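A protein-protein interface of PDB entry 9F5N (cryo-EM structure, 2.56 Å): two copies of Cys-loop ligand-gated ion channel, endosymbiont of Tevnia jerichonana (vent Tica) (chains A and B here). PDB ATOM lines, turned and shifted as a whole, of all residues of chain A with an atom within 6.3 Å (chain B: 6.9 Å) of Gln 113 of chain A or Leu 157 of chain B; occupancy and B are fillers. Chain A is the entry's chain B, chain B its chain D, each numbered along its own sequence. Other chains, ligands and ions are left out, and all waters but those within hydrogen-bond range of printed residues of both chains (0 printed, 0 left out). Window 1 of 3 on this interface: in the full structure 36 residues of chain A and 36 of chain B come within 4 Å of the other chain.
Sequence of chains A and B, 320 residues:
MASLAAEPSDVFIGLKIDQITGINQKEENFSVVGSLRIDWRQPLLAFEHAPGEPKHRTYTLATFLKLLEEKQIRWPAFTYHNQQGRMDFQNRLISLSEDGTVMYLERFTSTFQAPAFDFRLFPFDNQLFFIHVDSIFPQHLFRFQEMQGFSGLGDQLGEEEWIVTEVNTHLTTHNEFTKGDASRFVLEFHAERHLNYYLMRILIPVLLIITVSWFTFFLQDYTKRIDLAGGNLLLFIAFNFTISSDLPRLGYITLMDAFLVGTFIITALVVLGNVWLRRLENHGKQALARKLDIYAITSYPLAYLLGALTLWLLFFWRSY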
ATOM      1  N   GLU A  28       9.174  -7.210 -12.783  1.00  0.00           N
ATOM      2  CA  GLU A  28       9.215  -7.935 -11.515  1.00  0.00           C
ATOM      3  C   GLU A  28      10.254  -9.054 -11.543  1.00  0.00           C
ATOM      4  O   GLU A  28       9.972 -10.214 -11.251  1.00  0.00           O
ATOM      5  CB  GLU A  28       7.836  -8.470 -11.151  1.00  0.00           C
ATOM      6  CG  GLU A  28       6.883  -7.405 -10.650  1.00  0.00           C
ATOM      7  CD  GLU A  28       5.717  -7.977  -9.881  1.00  0.00           C
ATOM      8  OE1 GLU A  28       5.710  -9.195  -9.629  1.00  0.00           O
ATOM      9  OE2 GLU A  28       4.802  -7.208  -9.522  1.00  0.00           O
ATOM     10  N   ASN A  29      11.476  -8.694 -11.904  1.00  0.00           N
ATOM     11  CA  ASN A  29      12.586  -9.627 -11.881  1.00  0.00           C
ATOM     12  C   ASN A  29      13.830  -8.879 -11.437  1.00  0.00           C
ATOM     13  O   ASN A  29      13.831  -7.658 -11.308  1.00  0.00           O
ATOM     14  CB  ASN A  29      12.775 -10.325 -13.238  1.00  0.00           C
ATOM     15  CG  ASN A  29      13.114  -9.371 -14.368  1.00  0.00           C
ATOM     16  OD1 ASN A  29      13.887  -8.438 -14.210  1.00  0.00           O
ATOM     17  ND2 ASN A  29      12.552  -9.627 -15.525  1.00  0.00           N
ATOM     18  N   PHE A  30      14.890  -9.628 -11.173  1.00  0.00           N
ATOM     19  CA  PHE A  30      16.182  -9.043 -10.863  1.00  0.00           C
ATOM     20  C   PHE A  30      17.253  -9.931 -11.474  1.00  0.00           C
ATOM     21  O   PHE A  30      17.051 -11.133 -11.629  1.00  0.00           O
ATOM     22  CB  PHE A  30      16.385  -8.873  -9.351  1.00  0.00           C
ATOM     23  CG  PHE A  30      16.506 -10.168  -8.596  1.00  0.00           C
ATOM     24  CD1 PHE A  30      15.393 -10.924  -8.305  1.00  0.00           C
ATOM     25  CD2 PHE A  30      17.734 -10.615  -8.161  1.00  0.00           C
ATOM     26  CE1 PHE A  30      15.506 -12.103  -7.610  1.00  0.00           C
ATOM     27  CE2 PHE A  30      17.847 -11.792  -7.469  1.00  0.00           C
ATOM     28  CZ  PHE A  30      16.735 -12.533  -7.191  1.00  0.00           C
ATOM     29  N   HIS A  81      15.032 -22.747  -9.722  1.00  0.00           N
ATOM     30  CA  HIS A  81      13.601 -22.885  -9.946  1.00  0.00           C
ATOM     31  C   HIS A  81      12.977 -21.603 -10.485  1.00  0.00           C
ATOM     32  O   HIS A  81      12.074 -21.661 -11.324  1.00  0.00           O
ATOM     33  CB  HIS A  81      12.895 -23.321  -8.674  1.00  0.00           C
ATOM     34  CG  HIS A  81      11.432 -23.563  -8.869  1.00  0.00           C
ATOM     35  ND1 HIS A  81      10.950 -24.612  -9.618  1.00  0.00           N
ATOM     36  CD2 HIS A  81      10.348 -22.871  -8.449  1.00  0.00           C
ATOM     37  CE1 HIS A  81       9.632 -24.564  -9.640  1.00  0.00           C
ATOM     38  NE2 HIS A  81       9.241 -23.521  -8.934  1.00  0.00           N
ATOM     39  N   ASN A  82      13.435 -20.441 -10.026  1.00  0.00           N
ATOM     40  CA  ASN A  82      12.870 -19.172 -10.454  1.00  0.00           C
ATOM     41  C   ASN A  82      13.767 -18.426 -11.439  1.00  0.00           C
ATOM     42  O   ASN A  82      13.607 -17.216 -11.613  1.00  0.00           O
ATOM     43  CB  ASN A  82      12.538 -18.297  -9.240  1.00  0.00           C
ATOM     44  CG  ASN A  82      13.760 -17.884  -8.449  1.00  0.00           C
ATOM     45  OD1 ASN A  82      14.643 -18.692  -8.176  1.00  0.00           O
ATOM     46  ND2 ASN A  82      13.818 -16.621  -8.080  1.00  0.00           N
ATOM     47  N   GLN A  83      14.693 -19.118 -12.090  1.00  0.00           N
ATOM     48  CA  GLN A  83      15.425 -18.521 -13.194  1.00  0.00           C
ATOM     49  C   GLN A  83      14.488 -18.270 -14.368  1.00  0.00           C
ATOM     50  O   GLN A  83      13.617 -19.086 -14.675  1.00  0.00           O
ATOM     51  CB  GLN A  83      16.581 -19.419 -13.636  1.00  0.00           C
ATOM     52  CG  GLN A  83      16.909 -19.293 -15.110  1.00  0.00           C
ATOM     53  CD  GLN A  83      18.047 -20.173 -15.561  1.00  0.00           C
ATOM     54  OE1 GLN A  83      18.537 -21.014 -14.818  1.00  0.00           O
ATOM     55  NE2 GLN A  83      18.473 -19.982 -16.794  1.00  0.00           N
ATOM     56  N   GLN A  84      14.673 -17.144 -15.038  1.00  0.00           N
ATOM     57  CA  GLN A  84      13.950 -16.897 -16.272  1.00  0.00           C
ATOM     58  C   GLN A  84      14.919 -16.399 -17.334  1.00  0.00           C
ATOM     59  O   GLN A  84      15.762 -15.545 -17.062  1.00  0.00           O
ATOM     60  CB  GLN A  84      12.773 -15.935 -16.044  1.00  0.00           C
ATOM     61  CG  GLN A  84      13.104 -14.592 -15.519  1.00  0.00           C
ATOM     62  CD  GLN A  84      11.885 -13.714 -15.363  1.00  0.00           C
ATOM     63  OE1 GLN A  84      10.893 -14.091 -14.742  1.00  0.00           O
ATOM     64  NE2 GLN A  84      11.940 -12.541 -15.966  1.00  0.00           N
ATOM     65  N   THR A 111      18.886 -13.835 -14.930  1.00  0.00           N
ATOM     66  CA  THR A 111      17.740 -13.128 -14.386  1.00  0.00           C
ATOM     67  C   THR A 111      16.874 -14.106 -13.600  1.00  0.00           C
ATOM     68  O   THR A 111      16.820 -15.295 -13.909  1.00  0.00           O
ATOM     69  CB  THR A 111      16.932 -12.464 -15.506  1.00  0.00           C
ATOM     70  OG1 THR A 111      17.756 -11.523 -16.195  1.00  0.00           O
ATOM     71  CG2 THR A 111      15.741 -11.740 -14.967  1.00  0.00           C
ATOM     72  N   PHE A 112      16.233 -13.602 -12.550  1.00  0.00           N
ATOM     73  CA  PHE A 112      15.399 -14.400 -11.661  1.00  0.00           C
ATOM     74  C   PHE A 112      14.082 -13.690 -11.412  1.00  0.00           C
ATOM     75  O   PHE A 112      14.040 -12.465 -11.300  1.00  0.00           O
ATOM     76  CB  PHE A 112      16.092 -14.674 -10.312  1.00  0.00           C
ATOM     77  CG  PHE A 112      17.246 -15.621 -10.408  1.00  0.00           C
ATOM     78  CD1 PHE A 112      18.511 -15.156 -10.679  1.00  0.00           C
ATOM     79  CD2 PHE A 112      17.061 -16.976 -10.239  1.00  0.00           C
ATOM     80  CE1 PHE A 112      19.574 -16.025 -10.789  1.00  0.00           C
ATOM     81  CE2 PHE A 112      18.117 -17.843 -10.353  1.00  0.00           C
ATOM     82  CZ  PHE A 112      19.375 -17.360 -10.622  1.00  0.00           C
ATOM     83  N   GLN A 113      13.014 -14.474 -11.324  1.00  0.00           N
ATOM     84  CA  GLN A 113      11.700 -13.943 -11.007  1.00  0.00           C
ATOM     85  C   GLN A 113      11.676 -13.381  -9.591  1.00  0.00           C
ATOM     86  O   GLN A 113      12.336 -13.887  -8.686  1.00  0.00           O
ATOM     87  CB  GLN A 113      10.648 -15.038 -11.157  1.00  0.00           C
ATOM     88  CG  GLN A 113       9.222 -14.585 -10.966  1.00  0.00           C
ATOM     89  CD  GLN A 113       8.281 -15.747 -10.797  1.00  0.00           C
ATOM     90  OE1 GLN A 113       8.633 -16.749 -10.198  1.00  0.00           O
ATOM     91  NE2 GLN A 113       7.083 -15.622 -11.327  1.00  0.00           N
ATOM     92  N   ALA A 114      10.893 -12.325  -9.405  1.00  0.00           N
ATOM     93  CA  ALA A 114      10.689 -11.700  -8.101  1.00  0.00           C
ATOM     94  C   ALA A 114       9.197 -11.640  -7.847  1.00  0.00           C
ATOM     95  O   ALA A 114       8.586 -10.566  -7.890  1.00  0.00           O
ATOM     96  CB  ALA A 114      11.315 -10.308  -8.039  1.00  0.00           C
ATOM     97  N   PRO A 115       8.565 -12.782  -7.574  1.00  0.00           N
ATOM     98  CA  PRO A 115       7.106 -12.798  -7.465  1.00  0.00           C
ATOM     99  C   PRO A 115       6.577 -12.270  -6.142  1.00  0.00           C
ATOM    100  O   PRO A 115       5.356 -12.169  -5.983  1.00  0.00           O
ATOM    101  CB  PRO A 115       6.774 -14.278  -7.654  1.00  0.00           C
ATOM    102  CG  PRO A 115       7.953 -14.971  -7.102  1.00  0.00           C
ATOM    103  CD  PRO A 115       9.146 -14.117  -7.355  1.00  0.00           C
ATOM    104  N   ALA A 116       7.444 -11.909  -5.206  1.00  0.00           N
ATOM    105  CA  ALA A 116       7.024 -11.318  -3.948  1.00  0.00           C
ATOM    106  C   ALA A 116       6.953  -9.795  -3.986  1.00  0.00           C
ATOM    107  O   ALA A 116       6.617  -9.193  -2.964  1.00  0.00           O
ATOM    108  CB  ALA A 116       7.958 -11.756  -2.817  1.00  0.00           C
ATOM    109  N   PHE A 129      13.708 -10.759  -2.142  1.00  0.00           N
ATOM    110  CA  PHE A 129      14.332 -11.362  -3.311  1.00  0.00           C
ATOM    111  C   PHE A 129      14.922 -12.700  -2.897  1.00  0.00           C
ATOM    112  O   PHE A 129      15.531 -12.805  -1.831  1.00  0.00           O
ATOM    113  CB  PHE A 129      15.420 -10.459  -3.884  1.00  0.00           C
ATOM    114  CG  PHE A 129      14.961  -9.063  -4.162  1.00  0.00           C
ATOM    115  CD1 PHE A 129      14.354  -8.743  -5.360  1.00  0.00           C
ATOM    116  CD2 PHE A 129      15.113  -8.073  -3.212  1.00  0.00           C
ATOM    117  CE1 PHE A 129      13.930  -7.461  -5.603  1.00  0.00           C
ATOM    118  CE2 PHE A 129      14.690  -6.798  -3.449  1.00  0.00           C
ATOM    119  CZ  PHE A 129      14.100  -6.484  -4.641  1.00  0.00           C
ATOM    120  N   PHE A 130      14.732 -13.721  -3.722  1.00  0.00           N
ATOM    121  CA  PHE A 130      15.280 -15.027  -3.407  1.00  0.00           C
ATOM    122  C   PHE A 130      15.730 -15.727  -4.677  1.00  0.00           C
ATOM    123  O   PHE A 130      15.306 -15.400  -5.782  1.00  0.00           O
ATOM    124  CB  PHE A 130      14.284 -15.915  -2.652  1.00  0.00           C
ATOM    125  CG  PHE A 130      12.987 -16.125  -3.366  1.00  0.00           C
ATOM    126  CD1 PHE A 130      12.862 -17.111  -4.329  1.00  0.00           C
ATOM    127  CD2 PHE A 130      11.883 -15.359  -3.059  1.00  0.00           C
ATOM    128  CE1 PHE A 130      11.672 -17.312  -4.979  1.00  0.00           C
ATOM    129  CE2 PHE A 130      10.687 -15.560  -3.712  1.00  0.00           C
ATOM    130  CZ  PHE A 130      10.583 -16.541  -4.670  1.00  0.00           C
ATOM    131  N   ILE B  17       3.446 -24.970 -16.669  1.00  0.00           N
ATOM    132  CA  ILE B  17       3.851 -23.574 -16.764  1.00  0.00           C
ATOM    133  C   ILE B  17       4.095 -23.054 -15.357  1.00  0.00           C
ATOM    134  O   ILE B  17       3.183 -23.025 -14.526  1.00  0.00           O
ATOM    135  CB  ILE B  17       2.812 -22.720 -17.500  1.00  0.00           C
ATOM    136  CG1 ILE B  17       2.802 -23.057 -18.986  1.00  0.00           C
ATOM    137  CG2 ILE B  17       3.131 -21.236 -17.346  1.00  0.00           C
ATOM    138  CD1 ILE B  17       1.712 -22.353 -19.748  1.00  0.00           C
ATOM    139  N   ASP B  18       5.331 -22.650 -15.088  1.00  0.00           N
ATOM    140  CA  ASP B  18       5.712 -22.163 -13.773  1.00  0.00           C
ATOM    141  C   ASP B  18       5.742 -20.650 -13.678  1.00  0.00           C
ATOM    142  O   ASP B  18       5.436 -20.105 -12.619  1.00  0.00           O
ATOM    143  CB  ASP B  18       7.080 -22.723 -13.386  1.00  0.00           C
ATOM    144  CG  ASP B  18       7.042 -24.209 -13.147  1.00  0.00           C
ATOM    145  OD1 ASP B  18       6.484 -24.631 -12.111  1.00  0.00           O
ATOM    146  OD2 ASP B  18       7.555 -24.964 -13.999  1.00  0.00           O
ATOM    147  N   GLN B  19       6.097 -19.957 -14.748  1.00  0.00           N
ATOM    148  CA  GLN B  19       6.095 -18.508 -14.760  1.00  0.00           C
ATOM    149  C   GLN B  19       5.447 -18.013 -16.038  1.00  0.00           C
ATOM    150  O   GLN B  19       5.533 -18.654 -17.084  1.00  0.00           O
ATOM    151  CB  GLN B  19       7.515 -17.929 -14.647  1.00  0.00           C
ATOM    152  CG  GLN B  19       8.331 -18.438 -13.476  1.00  0.00           C
ATOM    153  CD  GLN B  19       9.779 -18.019 -13.556  1.00  0.00           C
ATOM    154  OE1 GLN B  19      10.085 -16.917 -13.987  1.00  0.00           O
ATOM    155  NE2 GLN B  19      10.672 -18.894 -13.151  1.00  0.00           N
ATOM    156  N   ILE B  20       4.783 -16.875 -15.940  1.00  0.00           N
ATOM    157  CA  ILE B  20       4.476 -16.051 -17.096  1.00  0.00           C
ATOM    158  C   ILE B  20       5.383 -14.840 -16.989  1.00  0.00           C
ATOM    159  O   ILE B  20       5.085 -13.881 -16.271  1.00  0.00           O
ATOM    160  CB  ILE B  20       2.997 -15.667 -17.172  1.00  0.00           C
ATOM    161  CG1 ILE B  20       2.170 -16.900 -17.486  1.00  0.00           C
ATOM    162  CG2 ILE B  20       2.765 -14.609 -18.236  1.00  0.00           C
ATOM    163  CD1 ILE B  20       0.747 -16.772 -17.102  1.00  0.00           C
ATOM    164  N   THR B  21       6.513 -14.897 -17.686  1.00  0.00           N
ATOM    165  CA  THR B  21       7.471 -13.809 -17.628  1.00  0.00           C
ATOM    166  C   THR B  21       6.949 -12.557 -18.310  1.00  0.00           C
ATOM    167  O   THR B  21       7.405 -11.457 -17.991  1.00  0.00           O
ATOM    168  CB  THR B  21       8.800 -14.240 -18.246  1.00  0.00           C
ATOM    169  OG1 THR B  21       8.656 -14.386 -19.658  1.00  0.00           O
ATOM    170  CG2 THR B  21       9.247 -15.569 -17.658  1.00  0.00           C
ATOM    171  N   GLY B  22       5.998 -12.692 -19.221  1.00  0.00           N
ATOM    172  CA  GLY B  22       5.424 -11.524 -19.839  1.00  0.00           C
ATOM    173  C   GLY B  22       4.359 -11.847 -20.856  1.00  0.00           C
ATOM    174  O   GLY B  22       4.396 -12.890 -21.503  1.00  0.00           O
ATOM    175  N   VAL B  33       8.144 -19.543 -18.365  1.00  0.00           N
ATOM    176  CA  VAL B  33       9.087 -20.533 -17.878  1.00  0.00           C
ATOM    177  C   VAL B  33       8.252 -21.755 -17.538  1.00  0.00           C
ATOM    178  O   VAL B  33       7.297 -21.656 -16.767  1.00  0.00           O
ATOM    179  CB  VAL B  33       9.873 -20.035 -16.655  1.00  0.00           C
ATOM    180  CG1 VAL B  33      10.805 -21.111 -16.159  1.00  0.00           C
ATOM    181  CG2 VAL B  33      10.637 -18.753 -16.968  1.00  0.00           C
ATOM    182  N   GLY B 152      -0.465 -28.176 -16.229  1.00  0.00           N
ATOM    183  CA  GLY B 152      -1.255 -27.080 -15.734  1.00  0.00           C
ATOM    184  C   GLY B 152      -0.451 -25.820 -15.554  1.00  0.00           C
ATOM    185  O   GLY B 152       0.554 -25.606 -16.234  1.00  0.00           O
ATOM    186  N   LEU B 153      -0.900 -24.979 -14.638  1.00  0.00           N
ATOM    187  CA  LEU B 153      -0.248 -23.723 -14.325  1.00  0.00           C
ATOM    188  C   LEU B 153       0.147 -23.736 -12.855  1.00  0.00           C
ATOM    189  O   LEU B 153      -0.433 -24.465 -12.049  1.00  0.00           O
ATOM    190  CB  LEU B 153      -1.164 -22.542 -14.661  1.00  0.00           C
ATOM    191  CG  LEU B 153      -0.899 -21.896 -16.027  1.00  0.00           C
ATOM    192  CD1 LEU B 153      -0.949 -22.895 -17.159  1.00  0.00           C
ATOM    193  CD2 LEU B 153      -1.851 -20.757 -16.311  1.00  0.00           C
ATOM    194  N   GLY B 154       1.167 -22.958 -12.519  1.00  0.00           N
ATOM    195  CA  GLY B 154       1.765 -23.000 -11.203  1.00  0.00           C
ATOM    196  C   GLY B 154       1.101 -22.060 -10.220  1.00  0.00           C
ATOM    197  O   GLY B 154       0.101 -21.401 -10.508  1.00  0.00           O
ATOM    198  N   ASP B 155       1.700 -21.984  -9.036  1.00  0.00           N
ATOM    199  CA  ASP B 155       1.183 -21.157  -7.957  1.00  0.00           C
ATOM    200  C   ASP B 155       1.733 -19.736  -7.977  1.00  0.00           C
ATOM    201  O   ASP B 155       1.047 -18.817  -7.517  1.00  0.00           O
ATOM    202  CB  ASP B 155       1.478 -21.821  -6.604  1.00  0.00           C
ATOM    203  CG  ASP B 155       2.964 -22.070  -6.376  1.00  0.00           C
ATOM    204  OD1 ASP B 155       3.568 -22.859  -7.133  1.00  0.00           O
ATOM    205  OD2 ASP B 155       3.528 -21.473  -5.437  1.00  0.00           O
ATOM    206  N   GLN B 156       2.938 -19.525  -8.502  1.00  0.00           N
ATOM    207  CA  GLN B 156       3.548 -18.199  -8.597  1.00  0.00           C
ATOM    208  C   GLN B 156       3.844 -17.905 -10.061  1.00  0.00           C
ATOM    209  O   GLN B 156       4.972 -18.062 -10.518  1.00  0.00           O
ATOM    210  CB  GLN B 156       4.812 -18.126  -7.776  1.00  0.00           C
ATOM    211  CG  GLN B 156       4.639 -18.324  -6.295  1.00  0.00           C
ATOM    212  CD  GLN B 156       5.868 -17.903  -5.513  1.00  0.00           C
ATOM    213  OE1 GLN B 156       5.772 -17.156  -4.539  1.00  0.00           O
ATOM    214  NE2 GLN B 156       7.035 -18.381  -5.938  1.00  0.00           N
ATOM    215  N   LEU B 157       2.838 -17.440 -10.792  1.00  0.00           N
ATOM    216  CA  LEU B 157       3.057 -17.159 -12.200  1.00  0.00           C
ATOM    217  C   LEU B 157       3.745 -15.829 -12.417  1.00  0.00           C
ATOM    218  O   LEU B 157       4.311 -15.615 -13.488  1.00  0.00           O
ATOM    219  CB  LEU B 157       1.739 -17.192 -12.967  1.00  0.00           C
ATOM    220  CG  LEU B 157       1.033 -18.546 -12.991  1.00  0.00           C
ATOM    221  CD1 LEU B 157      -0.278 -18.405 -13.709  1.00  0.00           C
ATOM    222  CD2 LEU B 157       1.899 -19.595 -13.650  1.00  0.00           C
ATOM    223  N   GLY B 158       3.706 -14.941 -11.429  1.00  0.00           N
ATOM    224  CA  GLY B 158       4.406 -13.683 -11.509  1.00  0.00           C
ATOM    225  C   GLY B 158       3.798 -12.664 -12.442  1.00  0.00           C
ATOM    226  O   GLY B 158       4.463 -11.689 -12.789  1.00  0.00           O
ATOM    227  N   GLU B 159       2.557 -12.860 -12.859  1.00  0.00           N
ATOM    228  CA  GLU B 159       1.878 -11.956 -13.774  1.00  0.00           C
ATOM    229  C   GLU B 159       0.911 -11.087 -12.981  1.00  0.00           C
ATOM    230  O   GLU B 159       0.061 -11.605 -12.254  1.00  0.00           O
ATOM    231  CB  GLU B 159       1.141 -12.744 -14.862  1.00  0.00           C
ATOM    232  CG  GLU B 159       0.296 -11.924 -15.805  1.00  0.00           C
ATOM    233  CD  GLU B 159       1.083 -10.848 -16.523  1.00  0.00           C
ATOM    234  OE1 GLU B 159       1.919 -11.189 -17.388  1.00  0.00           O
ATOM    235  OE2 GLU B 159       0.859  -9.663 -16.231  1.00  0.00           O
ATOM    236  N   GLU B 160       1.055  -9.770 -13.115  1.00  0.00           N
ATOM    237  CA  GLU B 160       0.308  -8.813 -12.307  1.00  0.00           C
ATOM    238  C   GLU B 160      -0.928  -8.260 -13.005  1.00  0.00           C
ATOM    239  O   GLU B 160      -1.940  -8.026 -12.345  1.00  0.00           O
ATOM    240  CB  GLU B 160       1.209  -7.647 -11.894  1.00  0.00           C
ATOM    241  CG  GLU B 160       2.237  -7.973 -10.840  1.00  0.00           C
ATOM    242  CD  GLU B 160       1.651  -8.052  -9.441  1.00  0.00           C
ATOM    243  OE1 GLU B 160       0.421  -8.195  -9.305  1.00  0.00           O
ATOM    244  OE2 GLU B 160       2.428  -7.951  -8.469  1.00  0.00           O
ATOM    245  N   VAL B 164      -5.570 -15.647 -14.504  1.00  0.00           N
ATOM    246  CA  VAL B 164      -5.961 -16.878 -15.175  1.00  0.00           C
ATOM    247  C   VAL B 164      -7.325 -17.322 -14.673  1.00  0.00           C
ATOM    248  O   VAL B 164      -7.555 -17.426 -13.464  1.00  0.00           O
ATOM    249  CB  VAL B 164      -4.904 -17.966 -14.951  1.00  0.00           C
ATOM    250  CG1 VAL B 164      -5.292 -19.239 -15.668  1.00  0.00           C
ATOM    251  CG2 VAL B 164      -3.556 -17.477 -15.426  1.00  0.00           C
ATOM    252  N   PHE B 189      -5.067 -21.922 -21.598  1.00  0.00           N
ATOM    253  CA  PHE B 189      -5.651 -21.229 -20.466  1.00  0.00           C
ATOM    254  C   PHE B 189      -6.240 -19.916 -20.945  1.00  0.00           C
ATOM    255  O   PHE B 189      -5.820 -19.360 -21.958  1.00  0.00           O
ATOM    256  CB  PHE B 189      -4.635 -21.001 -19.340  1.00  0.00           C
ATOM    257  CG  PHE B 189      -3.450 -20.166 -19.732  1.00  0.00           C
ATOM    258  CD1 PHE B 189      -2.373 -20.734 -20.382  1.00  0.00           C
ATOM    259  CD2 PHE B 189      -3.394 -18.824 -19.416  1.00  0.00           C
ATOM    260  CE1 PHE B 189      -1.276 -19.977 -20.725  1.00  0.00           C
ATOM    261  CE2 PHE B 189      -2.301 -18.068 -19.758  1.00  0.00           C
ATOM    262  CZ  PHE B 189      -1.238 -18.652 -20.411  1.00  0.00           C
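The side-chain carboxylate of Glu 28 of chain A sits close to the side-chain carboxylate of Glu 160 of chain B (2.7 Å).
O of Gln 83 of chain A sits at hydrogen-bond distance from NE2 of Gln 19 of chain B.
The side-chain amide oxygen (OE1) of Gln 19 of chain B lies close to the side-chain amide oxygen (OE1) of Gln 84 of chain A, 3.0 Å away.
The side-chain amide nitrogen of Gln 113 of chain A is in hydrogen-bond range of the backbone carbonyl oxygen of Gln 156 of chain B, 3.3 Å away.
The side-chain amide nitrogen (NE2) of Gln 113 of chain A sits close to the backbone NH (N) of Gly 158 of chain B, 3.4 Å away.
The backbone carbonyl oxygen (O) of Glu 28 of chain A lies within hydrogen-bond range of the backbone NH (N) of Ala 114 of chain A (3.0 Å).
The backbone carbonyl oxygen (O) of Phe 130 of chain A is in hydrogen-bond range of the side-chain amide nitrogen (ND2) of Asn 82 of chain A.
N of Gln 84 of chain A lies within hydrogen-bond range of O of Thr 111 of chain A (3.1 Å).
The backbone carbonyl oxygen of Val 33 of chain B sits at hydrogen-bond distance from the backbone NH of Asp 18 of chain B (2.8 Å).
The backbone NH of Gln 19 of chain B sits at hydrogen-bond distance from the backbone carbonyl oxygen of Val 33 of chain B (2.9 Å).
O of Leu 157 of chain B lies within hydrogen-bond range of N of Ile 20 of chain B, at 2.8 Å.
Among the printed residues, merely in contact across the chains: Gln 113 of chain A with Gln 19 of chain B (3.4 Å), Asn 82 of chain A with Gln 19 of chain B (3.5 Å), Gln 113 of chain A with Leu 157 of chain B (3.5 Å), His 81 of chain A with Gln 19 of chain B (3.6 Å), Gln 84 of chain A with Val 33 of chain B (3.7 Å), Gln 84 of chain A with Thr 21 of chain B (3.7 Å), Pro 115 of chain A with Gln 156 of chain B (3.7 Å) and Gln 83 of chain A with Val 33 of chain B (3.8 Å).
Phe 30 of chain A touches none of the printed residues of chain B.
Of the printed residues of chain B, His 81 of chain A touches Gln 19.
Gly 152 of chain B touches none of the printed residues of chain A.
Of the printed residues of chain A, Leu 157 of chain B touches Gln 113.
Of the printed residues of chain A, Gly 158 of chain B touches Gln 113.
Printed residues of chain A that touch a printed residue of chain B: Glu 28, His 81, Asn 82, Gln 83, Gln 84, Gln 113 and Pro 115.
Hydrophobic or aromatic side chains of chain A that line the printed part of chain B: Pro 115.
Along chain A the printed residues that touch a printed residue of chain B span positions 28 to 115.
Of the 18 printed residues of chain B, 7 touch a printed residue of chain A.
Hydrophobic or aromatic side chains of chain B that line the printed part of chain A: Val 33.
Among the printed residues, 13 pairs touch across the chains.
Among the printed residues, no Asp or Glu carboxylate lies within 4 Å of a Lys or Arg side-chain nitrogen of the other chain.
No position is printed for both chains.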
